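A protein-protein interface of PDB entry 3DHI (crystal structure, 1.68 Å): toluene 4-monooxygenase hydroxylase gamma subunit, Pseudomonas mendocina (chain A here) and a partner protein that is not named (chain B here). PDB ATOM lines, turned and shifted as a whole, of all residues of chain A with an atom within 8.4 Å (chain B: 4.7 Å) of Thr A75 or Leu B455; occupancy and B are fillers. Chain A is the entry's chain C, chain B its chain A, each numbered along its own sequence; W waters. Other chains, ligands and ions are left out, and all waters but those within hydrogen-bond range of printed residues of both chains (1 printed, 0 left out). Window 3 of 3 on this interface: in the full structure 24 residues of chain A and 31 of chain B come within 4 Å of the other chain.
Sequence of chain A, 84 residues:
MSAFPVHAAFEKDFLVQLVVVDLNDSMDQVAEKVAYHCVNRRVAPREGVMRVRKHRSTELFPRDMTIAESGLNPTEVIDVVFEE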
ATOM      1  N   ALA A   3      17.434  13.734  14.548  1.00  0.00           N
ATOM      2  CA  ALA A   3      17.637  12.284  14.728  1.00  0.00           C
ATOM      3  C   ALA A   3      18.694  11.830  13.733  1.00  0.00           C
ATOM      4  O   ALA A   3      18.655  12.220  12.569  1.00  0.00           O
ATOM      5  CB  ALA A   3      16.343  11.513  14.505  1.00  0.00           C
ATOM      6  N   PHE A   4      19.628  11.008  14.196  1.00  0.00           N
ATOM      7  CA  PHE A   4      20.770  10.605  13.384  1.00  0.00           C
ATOM      8  C   PHE A   4      21.075   9.131  13.664  1.00  0.00           C
ATOM      9  O   PHE A   4      21.625   8.811  14.707  1.00  0.00           O
ATOM     10  CB  PHE A   4      21.976  11.482  13.726  1.00  0.00           C
ATOM     11  CG  PHE A   4      23.135  11.357  12.769  1.00  0.00           C
ATOM     12  CD1 PHE A   4      23.339  12.315  11.777  1.00  0.00           C
ATOM     13  CD2 PHE A   4      24.040  10.299  12.877  1.00  0.00           C
ATOM     14  CE1 PHE A   4      24.407  12.215  10.895  1.00  0.00           C
ATOM     15  CE2 PHE A   4      25.117  10.193  12.008  1.00  0.00           C
ATOM     16  CZ  PHE A   4      25.294  11.148  11.009  1.00  0.00           C
ATOM     17  N   PRO A   5      20.711   8.229  12.735  1.00  0.00           N
ATOM     18  CA  PRO A   5      21.039   6.823  12.966  1.00  0.00           C
ATOM     19  C   PRO A   5      22.526   6.485  12.728  1.00  0.00           C
ATOM     20  O   PRO A   5      23.130   6.919  11.738  1.00  0.00           O
ATOM     21  CB  PRO A   5      20.129   6.085  11.974  1.00  0.00           C
ATOM     22  CG  PRO A   5      19.941   7.045  10.843  1.00  0.00           C
ATOM     23  CD  PRO A   5      19.983   8.434  11.463  1.00  0.00           C
ATOM     24  N   VAL A   6      23.116   5.744  13.661  1.00  0.00           N
ATOM     25  CA  VAL A   6      24.426   5.131  13.429  1.00  0.00           C
ATOM     26  C   VAL A   6      24.335   3.635  13.685  1.00  0.00           C
ATOM     27  O   VAL A   6      23.392   3.164  14.324  1.00  0.00           O
ATOM     28  CB  VAL A   6      25.552   5.719  14.322  1.00  0.00           C
ATOM     29  CG1 VAL A   6      25.823   7.177  13.957  1.00  0.00           C
ATOM     30  CG2 VAL A   6      25.224   5.559  15.805  1.00  0.00           C
ATOM     31  N   HIS A   7      25.319   2.890  13.186  1.00  0.00           N
ATOM     32  CA  HIS A   7      25.503   1.503  13.612  1.00  0.00           C
ATOM     33  C   HIS A   7      26.728   1.455  14.506  1.00  0.00           C
ATOM     34  O   HIS A   7      27.802   1.927  14.123  1.00  0.00           O
ATOM     35  CB  HIS A   7      25.653   0.583  12.390  1.00  0.00           C
ATOM     36  CG  HIS A   7      24.394   0.463  11.597  1.00  0.00           C
ATOM     37  ND1 HIS A   7      24.211   1.090  10.386  1.00  0.00           N
ATOM     38  CD2 HIS A   7      23.224  -0.162  11.880  1.00  0.00           C
ATOM     39  CE1 HIS A   7      22.991   0.839   9.945  1.00  0.00           C
ATOM     40  NE2 HIS A   7      22.377   0.073  10.827  1.00  0.00           N
ATOM     41  N   ALA A   8      26.576   0.914  15.709  1.00  0.00           N
ATOM     42  CA  ALA A   8      27.647   1.003  16.686  1.00  0.00           C
ATOM     43  C   ALA A   8      28.089  -0.346  17.239  1.00  0.00           C
ATOM     44  O   ALA A   8      27.257  -1.176  17.591  1.00  0.00           O
ATOM     45  CB  ALA A   8      27.224   1.977  17.838  1.00  0.00           C
ATOM     46  N   VAL A  16      26.997  -5.471  16.265  1.00  0.00           N
ATOM     47  CA  VAL A  16      26.819  -4.081  15.906  1.00  0.00           C
ATOM     48  C   VAL A  16      25.319  -3.815  15.999  1.00  0.00           C
ATOM     49  O   VAL A  16      24.504  -4.624  15.534  1.00  0.00           O
ATOM     50  CB  VAL A  16      27.304  -3.809  14.448  1.00  0.00           C
ATOM     51  CG1 VAL A  16      27.182  -2.327  14.093  1.00  0.00           C
ATOM     52  CG2 VAL A  16      28.754  -4.250  14.297  1.00  0.00           C
ATOM     53  N   LEU A  18      21.921  -0.879  15.793  1.00  0.00           N
ATOM     54  CA  LEU A  18      21.348   0.408  15.427  1.00  0.00           C
ATOM     55  C   LEU A  18      21.148   1.236  16.697  1.00  0.00           C
ATOM     56  O   LEU A  18      20.478   0.805  17.642  1.00  0.00           O
ATOM     57  CB  LEU A  18      20.017   0.227  14.692  1.00  0.00           C
ATOM     58  CG  LEU A  18      19.213   1.503  14.455  1.00  0.00           C
ATOM     59  CD1 LEU A  18      19.902   2.397  13.420  1.00  0.00           C
ATOM     60  CD2 LEU A  18      17.790   1.150  14.049  1.00  0.00           C
ATOM     61  N   VAL A  19      21.756   2.414  16.714  1.00  0.00           N
ATOM     62  CA  VAL A  19      21.537   3.368  17.806  1.00  0.00           C
ATOM     63  C   VAL A  19      21.228   4.718  17.177  1.00  0.00           C
ATOM     64  O   VAL A  19      22.022   5.246  16.384  1.00  0.00           O
ATOM     65  CB  VAL A  19      22.767   3.462  18.736  1.00  0.00           C
ATOM     66  CG1 VAL A  19      22.494   4.444  19.875  1.00  0.00           C
ATOM     67  CG2 VAL A  19      23.127   2.093  19.320  1.00  0.00           C
ATOM     68  N   VAL A  20      20.057   5.266  17.489  1.00  0.00           N
ATOM     69  CA  VAL A  20      19.654   6.539  16.894  1.00  0.00           C
ATOM     70  C   VAL A  20      20.060   7.654  17.861  1.00  0.00           C
ATOM     71  O   VAL A  20      19.532   7.749  18.976  1.00  0.00           O
ATOM     72  CB  VAL A  20      18.131   6.600  16.538  1.00  0.00           C
ATOM     73  CG1 VAL A  20      17.748   8.000  16.055  1.00  0.00           C
ATOM     74  CG2 VAL A  20      17.761   5.574  15.473  1.00  0.00           C
ATOM     75  N   LYS A  54      35.399   6.211  14.094  1.00  0.00           N
ATOM     76  CA  LYS A  54      34.878   5.525  12.906  1.00  0.00           C
ATOM     77  C   LYS A  54      35.313   4.068  12.967  1.00  0.00           C
ATOM     78  O   LYS A  54      36.409   3.756  13.421  1.00  0.00           O
ATOM     79  CB  LYS A  54      35.401   6.166  11.613  1.00  0.00           C
ATOM     80  CG  LYS A  54      34.715   7.467  11.240  1.00  0.00           C
ATOM     81  CD  LYS A  54      35.067   7.912   9.812  1.00  0.00           C
ATOM     82  CE  LYS A  54      34.488   6.967   8.756  1.00  0.00           C
ATOM     83  NZ  LYS A  54      32.988   6.922   8.771  1.00  0.00           N
ATOM     84  N   LEU A  72      30.611  12.537  10.012  1.00  0.00           N
ATOM     85  CA  LEU A  72      29.932  11.240   9.856  1.00  0.00           C
ATOM     86  C   LEU A  72      28.639  11.384   9.079  1.00  0.00           C
ATOM     87  O   LEU A  72      27.908  12.365   9.244  1.00  0.00           O
ATOM     88  CB  LEU A  72      29.619  10.592  11.218  1.00  0.00           C
ATOM     89  CG  LEU A  72      30.769  10.024  12.050  1.00  0.00           C
ATOM     90  CD1 LEU A  72      30.362   9.877  13.517  1.00  0.00           C
ATOM     91  CD2 LEU A  72      31.261   8.687  11.488  1.00  0.00           C
ATOM     92  N   ASN A  73      28.359  10.396   8.237  1.00  0.00           N
ATOM     93  CA  ASN A  73      27.116  10.332   7.499  1.00  0.00           C
ATOM     94  C   ASN A  73      26.158   9.374   8.197  1.00  0.00           C
ATOM     95  O   ASN A  73      26.606   8.438   8.849  1.00  0.00           O
ATOM     96  CB  ASN A  73      27.377   9.855   6.072  1.00  0.00           C
ATOM     97  CG  ASN A  73      28.240  10.827   5.285  1.00  0.00           C
ATOM     98  OD1 ASN A  73      27.859  11.975   5.070  1.00  0.00           O
ATOM     99  ND2 ASN A  73      29.406  10.365   4.846  1.00  0.00           N
ATOM    100  N   PRO A  74      24.842   9.609   8.061  1.00  0.00           N
ATOM    101  CA  PRO A  74      23.873   8.705   8.676  1.00  0.00           C
ATOM    102  C   PRO A  74      24.108   7.261   8.239  1.00  0.00           C
ATOM    103  O   PRO A  74      24.416   6.998   7.063  1.00  0.00           O
ATOM    104  CB  PRO A  74      22.531   9.211   8.135  1.00  0.00           C
ATOM    105  CG  PRO A  74      22.762  10.638   7.876  1.00  0.00           C
ATOM    106  CD  PRO A  74      24.175  10.725   7.369  1.00  0.00           C
ATOM    107  N   THR A  75      23.950   6.349   9.192  1.00  0.00           N
ATOM    108  CA  THR A  75      24.067   4.890   8.969  1.00  0.00           C
ATOM    109  C   THR A  75      25.508   4.412   8.772  1.00  0.00           C
ATOM    110  O   THR A  75      25.739   3.238   8.499  1.00  0.00           O
ATOM    111  CB  THR A  75      23.120   4.349   7.839  1.00  0.00           C
ATOM    112  OG1 THR A  75      23.658   4.644   6.538  1.00  0.00           O
ATOM    113  CG2 THR A  75      21.704   4.908   7.979  1.00  0.00           C
ATOM    114  N   GLU A  76      26.482   5.301   8.963  1.00  0.00           N
ATOM    115  CA  GLU A  76      27.874   4.858   9.028  1.00  0.00           C
ATOM    116  C   GLU A  76      28.130   4.086  10.326  1.00  0.00           C
ATOM    117  O   GLU A  76      27.370   4.218  11.294  1.00  0.00           O
ATOM    118  CB  GLU A  76      28.846   6.040   8.854  1.00  0.00           C
ATOM    119  CG  GLU A  76      28.912   6.534   7.408  1.00  0.00           C
ATOM    120  CD  GLU A  76      29.900   7.687   7.146  1.00  0.00           C
ATOM    121  OE1 GLU A  76      30.396   8.345   8.086  1.00  0.00           O
ATOM    122  OE2 GLU A  76      30.180   7.938   5.953  1.00  0.00           O
ATOM    123  N   VAL A  77      29.180   3.271  10.328  1.00  0.00           N
ATOM    124  CA  VAL A  77      29.522   2.436  11.477  1.00  0.00           C
ATOM    125  C   VAL A  77      30.575   3.110  12.351  1.00  0.00           C
ATOM    126  O   VAL A  77      31.601   3.575  11.845  1.00  0.00           O
ATOM    127  CB  VAL A  77      30.072   1.055  11.041  1.00  0.00           C
ATOM    128  CG1 VAL A  77      30.178   0.104  12.237  1.00  0.00           C
ATOM    129  CG2 VAL A  77      29.222   0.443   9.921  1.00  0.00           C
ATOM    130  N   ILE A  78      30.316   3.127  13.661  1.00  0.00           N
ATOM    131  CA  ILE A  78      31.262   3.619  14.670  1.00  0.00           C
ATOM    132  C   ILE A  78      31.577   2.529  15.706  1.00  0.00           C
ATOM    133  O   ILE A  78      30.771   1.607  15.909  1.00  0.00           O
ATOM    134  CB  ILE A  78      30.714   4.895  15.381  1.00  0.00           C
ATOM    135  CG1 ILE A  78      29.411   4.577  16.132  1.00  0.00           C
ATOM    136  CG2 ILE A  78      30.519   6.031  14.362  1.00  0.00           C
ATOM    137  CD1 ILE A  78      28.969   5.677  17.161  1.00  0.00           C
ATOM    138  N   LEU B 425      24.469   3.406   0.973  1.00  0.00           N
ATOM    139  CA  LEU B 425      25.460   2.724   1.815  1.00  0.00           C
ATOM    140  C   LEU B 425      24.939   1.371   2.287  1.00  0.00           C
ATOM    141  O   LEU B 425      23.892   1.294   2.944  1.00  0.00           O
ATOM    142  CB  LEU B 425      25.845   3.588   3.027  1.00  0.00           C
ATOM    143  CG  LEU B 425      26.976   3.060   3.919  1.00  0.00           C
ATOM    144  CD1 LEU B 425      28.265   2.897   3.150  1.00  0.00           C
ATOM    145  CD2 LEU B 425      27.234   3.985   5.136  1.00  0.00           C
ATOM    146  N   HIS B 427      25.985  -2.548   4.147  1.00  0.00           N
ATOM    147  CA  HIS B 427      26.887  -3.105   5.151  1.00  0.00           C
ATOM    148  C   HIS B 427      26.787  -4.615   5.097  1.00  0.00           C
ATOM    149  O   HIS B 427      25.678  -5.152   5.103  1.00  0.00           O
ATOM    150  CB  HIS B 427      26.516  -2.640   6.558  1.00  0.00           C
ATOM    151  CG  HIS B 427      26.492  -1.148   6.716  1.00  0.00           C
ATOM    152  ND1 HIS B 427      27.635  -0.385   6.678  1.00  0.00           N
ATOM    153  CD2 HIS B 427      25.462  -0.282   6.885  1.00  0.00           C
ATOM    154  CE1 HIS B 427      27.317   0.890   6.841  1.00  0.00           C
ATOM    155  NE2 HIS B 427      26.004   0.978   6.974  1.00  0.00           N
ATOM    156  N   VAL B 451      16.306  -3.708   8.687  1.00  0.00           N
ATOM    157  CA  VAL B 451      16.749  -2.440   9.304  1.00  0.00           C
ATOM    158  C   VAL B 451      16.554  -1.259   8.344  1.00  0.00           C
ATOM    159  O   VAL B 451      16.057  -0.179   8.731  1.00  0.00           O
ATOM    160  CB  VAL B 451      18.206  -2.533   9.798  1.00  0.00           C
ATOM    161  CG1 VAL B 451      18.722  -1.178  10.295  1.00  0.00           C
ATOM    162  CG2 VAL B 451      18.317  -3.548  10.905  1.00  0.00           C
ATOM    163  N   ASP B 452      16.909  -1.463   7.077  1.00  0.00           N
ATOM    164  CA  ASP B 452      16.678  -0.451   6.042  1.00  0.00           C
ATOM    165  C   ASP B 452      15.206  -0.055   5.981  1.00  0.00           C
ATOM    166  O   ASP B 452      14.885   1.130   5.857  1.00  0.00           O
ATOM    167  CB  ASP B 452      17.093  -0.954   4.664  1.00  0.00           C
ATOM    168  CG  ASP B 452      18.562  -1.330   4.570  1.00  0.00           C
ATOM    169  OD1 ASP B 452      19.446  -0.684   5.200  1.00  0.00           O
ATOM    170  OD2 ASP B 452      18.824  -2.287   3.813  1.00  0.00           O
ATOM    171  N   ARG B 453      14.317  -1.049   6.084  1.00  0.00           N
ATOM    172  CA  ARG B 453      12.862  -0.802   6.085  1.00  0.00           C
ATOM    173  C   ARG B 453      12.407  -0.007   7.317  1.00  0.00           C
ATOM    174  O   ARG B 453      11.568   0.899   7.219  1.00  0.00           O
ATOM    175  CB  ARG B 453      12.099  -2.130   5.996  1.00  0.00           C
ATOM    176  CG  ARG B 453      12.411  -2.906   4.723  1.00  0.00           C
ATOM    177  CD  ARG B 453      11.643  -4.217   4.655  1.00  0.00           C
ATOM    178  NE  ARG B 453      12.338  -5.152   3.773  1.00  0.00           N
ATOM    179  CZ  ARG B 453      11.848  -6.322   3.372  1.00  0.00           C
ATOM    180  NH1 ARG B 453      10.638  -6.732   3.766  1.00  0.00           N
ATOM    181  NH2 ARG B 453      12.584  -7.091   2.579  1.00  0.00           N
ATOM    182  N   PHE B 454      12.977  -0.341   8.467  1.00  0.00           N
ATOM    183  CA  PHE B 454      12.649   0.319   9.736  1.00  0.00           C
ATOM    184  C   PHE B 454      13.040   1.795   9.608  1.00  0.00           C
ATOM    185  O   PHE B 454      12.247   2.688   9.871  1.00  0.00           O
ATOM    186  CB  PHE B 454      13.419  -0.348  10.864  1.00  0.00           C
ATOM    187  CG  PHE B 454      13.004   0.088  12.239  1.00  0.00           C
ATOM    188  CD1 PHE B 454      11.857  -0.440  12.830  1.00  0.00           C
ATOM    189  CD2 PHE B 454      13.772   1.006  12.956  1.00  0.00           C
ATOM    190  CE1 PHE B 454      11.470  -0.058  14.109  1.00  0.00           C
ATOM    191  CE2 PHE B 454      13.384   1.412  14.247  1.00  0.00           C
ATOM    192  CZ  PHE B 454      12.235   0.868  14.824  1.00  0.00           C
ATOM    193  N   LEU B 455      14.255   2.031   9.125  1.00  0.00           N
ATOM    194  CA  LEU B 455      14.736   3.406   8.930  1.00  0.00           C
ATOM    195  C   LEU B 455      14.010   4.199   7.849  1.00  0.00           C
ATOM    196  O   LEU B 455      13.973   5.443   7.914  1.00  0.00           O
ATOM    197  CB  LEU B 455      16.238   3.397   8.668  1.00  0.00           C
ATOM    198  CG  LEU B 455      17.098   3.014   9.873  1.00  0.00           C
ATOM    199  CD1 LEU B 455      18.573   2.924   9.449  1.00  0.00           C
ATOM    200  CD2 LEU B 455      16.920   4.030  10.990  1.00  0.00           C
ATOM    201  N   ALA B 456      13.436   3.507   6.863  1.00  0.00           N
ATOM    202  CA  ALA B 456      12.736   4.168   5.762  1.00  0.00           C
ATOM    203  C   ALA B 456      11.258   4.468   6.044  1.00  0.00           C
ATOM    204  O   ALA B 456      10.579   5.038   5.194  1.00  0.00           O
ATOM    205  CB  ALA B 456      12.856   3.356   4.482  1.00  0.00           C
ATOM    206  N   GLY B 457      10.751   4.052   7.198  1.00  0.00           N
ATOM    207  CA  GLY B 457       9.339   4.291   7.528  1.00  0.00           C
ATOM    208  C   GLY B 457       8.391   3.242   6.956  1.00  0.00           C
ATOM    209  O   GLY B 457       7.196   3.485   6.787  1.00  0.00           O
HETATM  210  O   HOH W   1      23.471   1.932   5.679  1.00  0.00           O
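Among the printed residues, pairs that only touch across the chains: Pro A5 with Leu B455, His A7 with His B427, His A7 with Val B451, Thr A75 with Leu B425, Thr A75 with Leu B455, Glu A76 with Leu B425 and Val A77 with His B427.
The backbone carbonyl oxygen (O) of Pro A5 sits at hydrogen-bond distance from the backbone NH (N) of Thr A75 (2.7 Å).
O of Thr A75 lies within hydrogen-bond range of ND1 of His A7 (3.2 Å).
The backbone NH of His A7 lies within hydrogen-bond range of the backbone carbonyl oxygen of Glu A76 (3.1 Å).
O of His A7 lies within hydrogen-bond range of N of Ile A78, 2.8 Å away.
The side-chain amino group (NZ) of Lys A54 lies within salt-bridge range of the side-chain carboxylate (OE1) of Glu A76.
The side-chain amide nitrogen of Asn A73 is in hydrogen-bond range of the side-chain carboxylate of Glu A76, at 2.8 Å.
O of Thr A75 is in hydrogen-bond range of NE2 of His B427 (2.7 Å).
Phe A4 touches none of the printed residues of chain B.
Of the printed residues of chain B, Thr A75 touches Leu B425 (3.8 Å), His B427 (2.7 Å) and Leu B455 (3.99 Å).
Of the printed residues of chain B, Glu A76 touches Leu B425 (3.8 Å).
Of the printed residues of chain A, Leu B425 touches Thr A75 (3.8 Å) and Glu A76 (3.8 Å).
Of the printed residues of chain A, His B427 touches His A7 (3.9 Å), Thr A75 (2.7 Å) and Val A77 (3.6 Å).
Of the printed residues of chain A, Val B451 touches His A7 (3.9 Å).
Of the printed residues of chain A, Leu B455 touches Pro A5 and Thr A75.
Gly B457 touches none of the printed residues of chain A.
The nearest printed residue of chain A that does not touch Val B451 is Leu A18 (4.5 Å).
Of the 9 printed residues of chain B, 4 touch a printed residue of chain A.
Hydrophobic or aromatic side chains of chain B that line the printed part of chain A: Leu B425, His B427, Val B451 and Leu B455.
Along chain B the printed residues that touch a printed residue of chain A span positions 425 to 455.
Along chain A the printed residues that touch a printed residue of chain B span positions 5 to 77.
Water W1 lies within hydrogen-bond range of the backbone carbonyl oxygen (O) of Leu B425 (2.8 Å), the side-chain hydroxyl (OG1) of Thr A75 (2.9 Å) and a ring nitrogen (NE2) of His B427 (3.0 Å).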
